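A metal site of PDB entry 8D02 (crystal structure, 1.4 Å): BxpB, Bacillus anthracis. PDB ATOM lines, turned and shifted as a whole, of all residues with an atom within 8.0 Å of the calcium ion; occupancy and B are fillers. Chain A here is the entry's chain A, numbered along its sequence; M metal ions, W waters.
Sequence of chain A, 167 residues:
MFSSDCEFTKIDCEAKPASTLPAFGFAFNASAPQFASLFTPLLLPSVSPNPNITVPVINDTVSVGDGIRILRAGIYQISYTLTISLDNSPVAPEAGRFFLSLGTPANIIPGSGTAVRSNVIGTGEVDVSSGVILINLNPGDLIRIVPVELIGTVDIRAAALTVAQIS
The backbone NH (N) of Glu 94 lies within hydrogen-bond range of the side-chain amide oxygen (OD1) of Asn 88, at 3.5 Å.
The side-chain carboxylate (OD1) of Asp 87 is bound to the calcium ion.
The side-chain hydroxyl (OG1) of Thr 153 binds the calcium ion (2.4 Å).
O of Thr 153 is bound to the calcium ion (2.4 Å).
O of Ser 89 binds the calcium ion, 2.5 Å away.
Water W2 binds the calcium ion, 2.5 Å away.
The calcium ion is bound by the side-chain carboxylate (OE2) of Glu 94, at 2.5 Å.
The calcium ion is bound by OE1 of Glu 94 (2.5 Å).
Water W1 binds the calcium ion, at 2.5 Å.
The calcium ion has eight donor atoms within binding distance.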
ATOM      1  N   PHE A  35     -10.414  13.833   2.384  1.00  0.00           N
ATOM      2  CA  PHE A  35     -10.753  13.440   1.036  1.00  0.00           C
ATOM      3  C   PHE A  35     -11.785  14.392   0.471  1.00  0.00           C
ATOM      4  O   PHE A  35     -12.674  14.879   1.186  1.00  0.00           O
ATOM      5  CB  PHE A  35     -11.288  12.008   1.031  1.00  0.00           C
ATOM      6  CG  PHE A  35     -10.222  11.006   1.193  1.00  0.00           C
ATOM      7  CD1 PHE A  35      -9.412  10.665   0.132  1.00  0.00           C
ATOM      8  CD2 PHE A  35     -10.036  10.367   2.425  1.00  0.00           C
ATOM      9  CE1 PHE A  35      -8.413   9.730   0.260  1.00  0.00           C
ATOM     10  CE2 PHE A  35      -9.039   9.411   2.579  1.00  0.00           C
ATOM     11  CZ  PHE A  35      -8.222   9.101   1.501  1.00  0.00           C
ATOM     12  N   SER A  85      -2.982  14.514  -3.196  1.00  0.00           N
ATOM     13  CA  SER A  85      -2.393  13.193  -3.382  1.00  0.00           C
ATOM     14  C   SER A  85      -3.357  12.313  -4.214  1.00  0.00           C
ATOM     15  O   SER A  85      -4.540  12.149  -3.851  1.00  0.00           O
ATOM     16  CB  SER A  85      -2.098  12.577  -2.015  1.00  0.00           C
ATOM     17  OG  SER A  85      -1.717  11.212  -2.183  1.00  0.00           O
ATOM     18  N   LEU A  86      -2.871  11.846  -5.366  1.00  0.00           N
ATOM     19  CA  LEU A  86      -3.629  10.990  -6.306  1.00  0.00           C
ATOM     20  C   LEU A  86      -2.866   9.674  -6.380  1.00  0.00           C
ATOM     21  O   LEU A  86      -2.050   9.498  -7.305  1.00  0.00           O
ATOM     22  CB  LEU A  86      -3.701  11.695  -7.637  1.00  0.00           C
ATOM     23  CG  LEU A  86      -4.299  13.097  -7.678  1.00  0.00           C
ATOM     24  CD1 LEU A  86      -4.025  13.776  -9.062  1.00  0.00           C
ATOM     25  CD2 LEU A  86      -5.796  13.096  -7.357  1.00  0.00           C
ATOM     26  N   ASP A  87      -3.131   8.766  -5.429  1.00  0.00           N
ATOM     27  CA  ASP A  87      -2.298   7.590  -5.314  1.00  0.00           C
ATOM     28  C   ASP A  87      -2.715   6.466  -6.251  1.00  0.00           C
ATOM     29  O   ASP A  87      -2.046   5.421  -6.262  1.00  0.00           O
ATOM     30  CB  ASP A  87      -2.231   7.125  -3.871  1.00  0.00           C
ATOM     31  CG  ASP A  87      -3.589   6.692  -3.312  1.00  0.00           C
ATOM     32  OD1 ASP A  87      -4.584   6.655  -4.058  1.00  0.00           O
ATOM     33  OD2 ASP A  87      -3.662   6.395  -2.096  1.00  0.00           O
ATOM     34  N   ASN A  88      -3.775   6.615  -7.032  1.00  0.00           N
ATOM     35  CA  ASN A  88      -4.243   5.601  -7.958  1.00  0.00           C
ATOM     36  C   ASN A  88      -4.821   4.387  -7.237  1.00  0.00           C
ATOM     37  O   ASN A  88      -4.895   3.312  -7.844  1.00  0.00           O
ATOM     38  CB  ASN A  88      -3.208   5.235  -9.046  1.00  0.00           C
ATOM     39  CG  ASN A  88      -3.122   6.275 -10.117  1.00  0.00           C
ATOM     40  OD1 ASN A  88      -4.038   7.083 -10.264  1.00  0.00           O
ATOM     41  ND2 ASN A  88      -2.062   6.217 -10.913  1.00  0.00           N
ATOM     42  N   SER A  89      -5.249   4.547  -5.986  1.00  0.00           N
ATOM     43  CA  SER A  89      -6.025   3.513  -5.318  1.00  0.00           C
ATOM     44  C   SER A  89      -7.294   4.179  -4.803  1.00  0.00           C
ATOM     45  O   SER A  89      -7.233   5.254  -4.167  1.00  0.00           O
ATOM     46  CB  SER A  89      -5.216   2.964  -4.172  1.00  0.00           C
ATOM     47  OG  SER A  89      -6.032   2.036  -3.436  1.00  0.00           O
ATOM     48  N   PRO A  90      -8.463   3.570  -5.003  1.00  0.00           N
ATOM     49  CA  PRO A  90      -8.661   2.222  -5.561  1.00  0.00           C
ATOM     50  C   PRO A  90      -8.829   2.171  -7.084  1.00  0.00           C
ATOM     51  O   PRO A  90      -8.998   1.065  -7.629  1.00  0.00           O
ATOM     52  CB  PRO A  90      -9.976   1.804  -4.858  1.00  0.00           C
ATOM     53  CG  PRO A  90     -10.716   3.026  -4.732  1.00  0.00           C
ATOM     54  CD  PRO A  90      -9.718   4.168  -4.519  1.00  0.00           C
ATOM     55  N   VAL A  91      -8.819   3.309  -7.785  1.00  0.00           N
ATOM     56  CA  VAL A  91      -8.963   3.362  -9.236  1.00  0.00           C
ATOM     57  C   VAL A  91      -7.789   4.169  -9.771  1.00  0.00           C
ATOM     58  O   VAL A  91      -7.207   4.998  -9.065  1.00  0.00           O
ATOM     59  CB  VAL A  91     -10.276   4.049  -9.694  1.00  0.00           C
ATOM     60  CG1 VAL A  91     -11.540   3.293  -9.172  1.00  0.00           C
ATOM     61  CG2 VAL A  91     -10.307   5.554  -9.316  1.00  0.00           C
ATOM     62  N   PRO A  93      -6.963   6.396 -13.496  1.00  0.00           N
ATOM     63  CA  PRO A  93      -6.354   7.509 -12.758  1.00  0.00           C
ATOM     64  C   PRO A  93      -7.333   8.060 -11.731  1.00  0.00           C
ATOM     65  O   PRO A  93      -8.475   7.626 -11.644  1.00  0.00           O
ATOM     66  CB  PRO A  93      -6.092   8.555 -13.843  1.00  0.00           C
ATOM     67  CG  PRO A  93      -7.117   8.267 -14.887  1.00  0.00           C
ATOM     68  CD  PRO A  93      -7.331   6.782 -14.879  1.00  0.00           C
ATOM     69  N   GLU A  94      -6.853   9.011 -10.944  1.00  0.00           N
ATOM     70  CA  GLU A  94      -7.683   9.808 -10.037  1.00  0.00           C
ATOM     71  C   GLU A  94      -7.612  11.271 -10.497  1.00  0.00           C
ATOM     72  O   GLU A  94      -6.646  11.678 -11.148  1.00  0.00           O
ATOM     73  CB  GLU A  94      -7.273   9.643  -8.590  1.00  0.00           C
ATOM     74  CG  GLU A  94      -7.446   8.172  -8.163  1.00  0.00           C
ATOM     75  CD  GLU A  94      -7.166   7.934  -6.714  1.00  0.00           C
ATOM     76  OE1 GLU A  94      -6.046   8.238  -6.238  1.00  0.00           O
ATOM     77  OE2 GLU A  94      -8.066   7.435  -6.011  1.00  0.00           O
ATOM     78  N   ALA A  95      -8.653  12.039 -10.204  1.00  0.00           N
ATOM     79  CA  ALA A  95      -8.723  13.378 -10.757  1.00  0.00           C
ATOM     80  C   ALA A  95      -9.666  14.212  -9.929  1.00  0.00           C
ATOM     81  O   ALA A  95     -10.612  13.705  -9.320  1.00  0.00           O
ATOM     82  CB  ALA A  95      -9.274  13.323 -12.174  1.00  0.00           C
ATOM     83  N   ILE A 151     -12.780  11.883  -9.648  1.00  0.00           N
ATOM     84  CA  ILE A 151     -12.605  10.471  -9.966  1.00  0.00           C
ATOM     85  C   ILE A 151     -11.732   9.872  -8.898  1.00  0.00           C
ATOM     86  O   ILE A 151     -10.595  10.323  -8.704  1.00  0.00           O
ATOM     87  CB  ILE A 151     -11.957  10.243 -11.339  1.00  0.00           C
ATOM     88  CG1 ILE A 151     -12.733  10.899 -12.454  1.00  0.00           C
ATOM     89  CG2 ILE A 151     -11.772   8.752 -11.548  1.00  0.00           C
ATOM     90  CD1 ILE A 151     -11.974  10.844 -13.787  1.00  0.00           C
ATOM     91  N   GLY A 152     -12.251   8.871  -8.191  1.00  0.00           N
ATOM     92  CA  GLY A 152     -11.471   8.216  -7.171  1.00  0.00           C
ATOM     93  C   GLY A 152     -11.490   8.905  -5.828  1.00  0.00           C
ATOM     94  O   GLY A 152     -12.372   9.737  -5.496  1.00  0.00           O
ATOM     95  N   THR A 153     -10.496   8.550  -5.035  1.00  0.00           N
ATOM     96  CA  THR A 153     -10.320   9.121  -3.700  1.00  0.00           C
ATOM     97  C   THR A 153      -9.185  10.133  -3.781  1.00  0.00           C
ATOM     98  O   THR A 153      -7.996   9.761  -3.833  1.00  0.00           O
ATOM     99  CB  THR A 153     -10.094   8.064  -2.618  1.00  0.00           C
ATOM    100  OG1 THR A 153      -8.966   7.256  -2.964  1.00  0.00           O
ATOM    101  CG2 THR A 153     -11.327   7.139  -2.498  1.00  0.00           C
ATOM    102  N   VAL A 154      -9.555  11.407  -3.798  1.00  0.00           N
ATOM    103  CA  VAL A 154      -8.643  12.519  -4.022  1.00  0.00           C
ATOM    104  C   VAL A 154      -8.309  13.091  -2.640  1.00  0.00           C
ATOM    105  O   VAL A 154      -9.203  13.619  -1.959  1.00  0.00           O
ATOM    106  CB  VAL A 154      -9.286  13.553  -4.958  1.00  0.00           C
ATOM    107  CG1 VAL A 154      -8.386  14.764  -5.095  1.00  0.00           C
ATOM    108  CG2 VAL A 154      -9.516  12.893  -6.334  1.00  0.00           C
ATOM    109  N   ASP A 155      -7.091  12.883  -2.189  1.00  0.00           N
ATOM    110  CA  ASP A 155      -6.623  13.241  -0.855  1.00  0.00           C
ATOM    111  C   ASP A 155      -6.086  14.662  -0.814  1.00  0.00           C
ATOM    112  O   ASP A 155      -4.968  14.925  -1.306  1.00  0.00           O
ATOM    113  CB  ASP A 155      -5.505  12.261  -0.528  1.00  0.00           C
ATOM    114  CG  ASP A 155      -5.142  12.191   0.924  1.00  0.00           C
ATOM    115  OD1 ASP A 155      -5.596  13.047   1.686  1.00  0.00           O
ATOM    116  OD2 ASP A 155      -4.230  11.388   1.239  1.00  0.00           O
HETATM  117 CA    CA M   1      -6.774   7.661  -3.922  1.00  0.00          CA
HETATM  118  O   HOH W   1      -5.127   9.398  -3.209  1.00  0.00           O
HETATM  119  O   HOH W   2      -6.213   7.124  -1.582  1.00  0.00           O
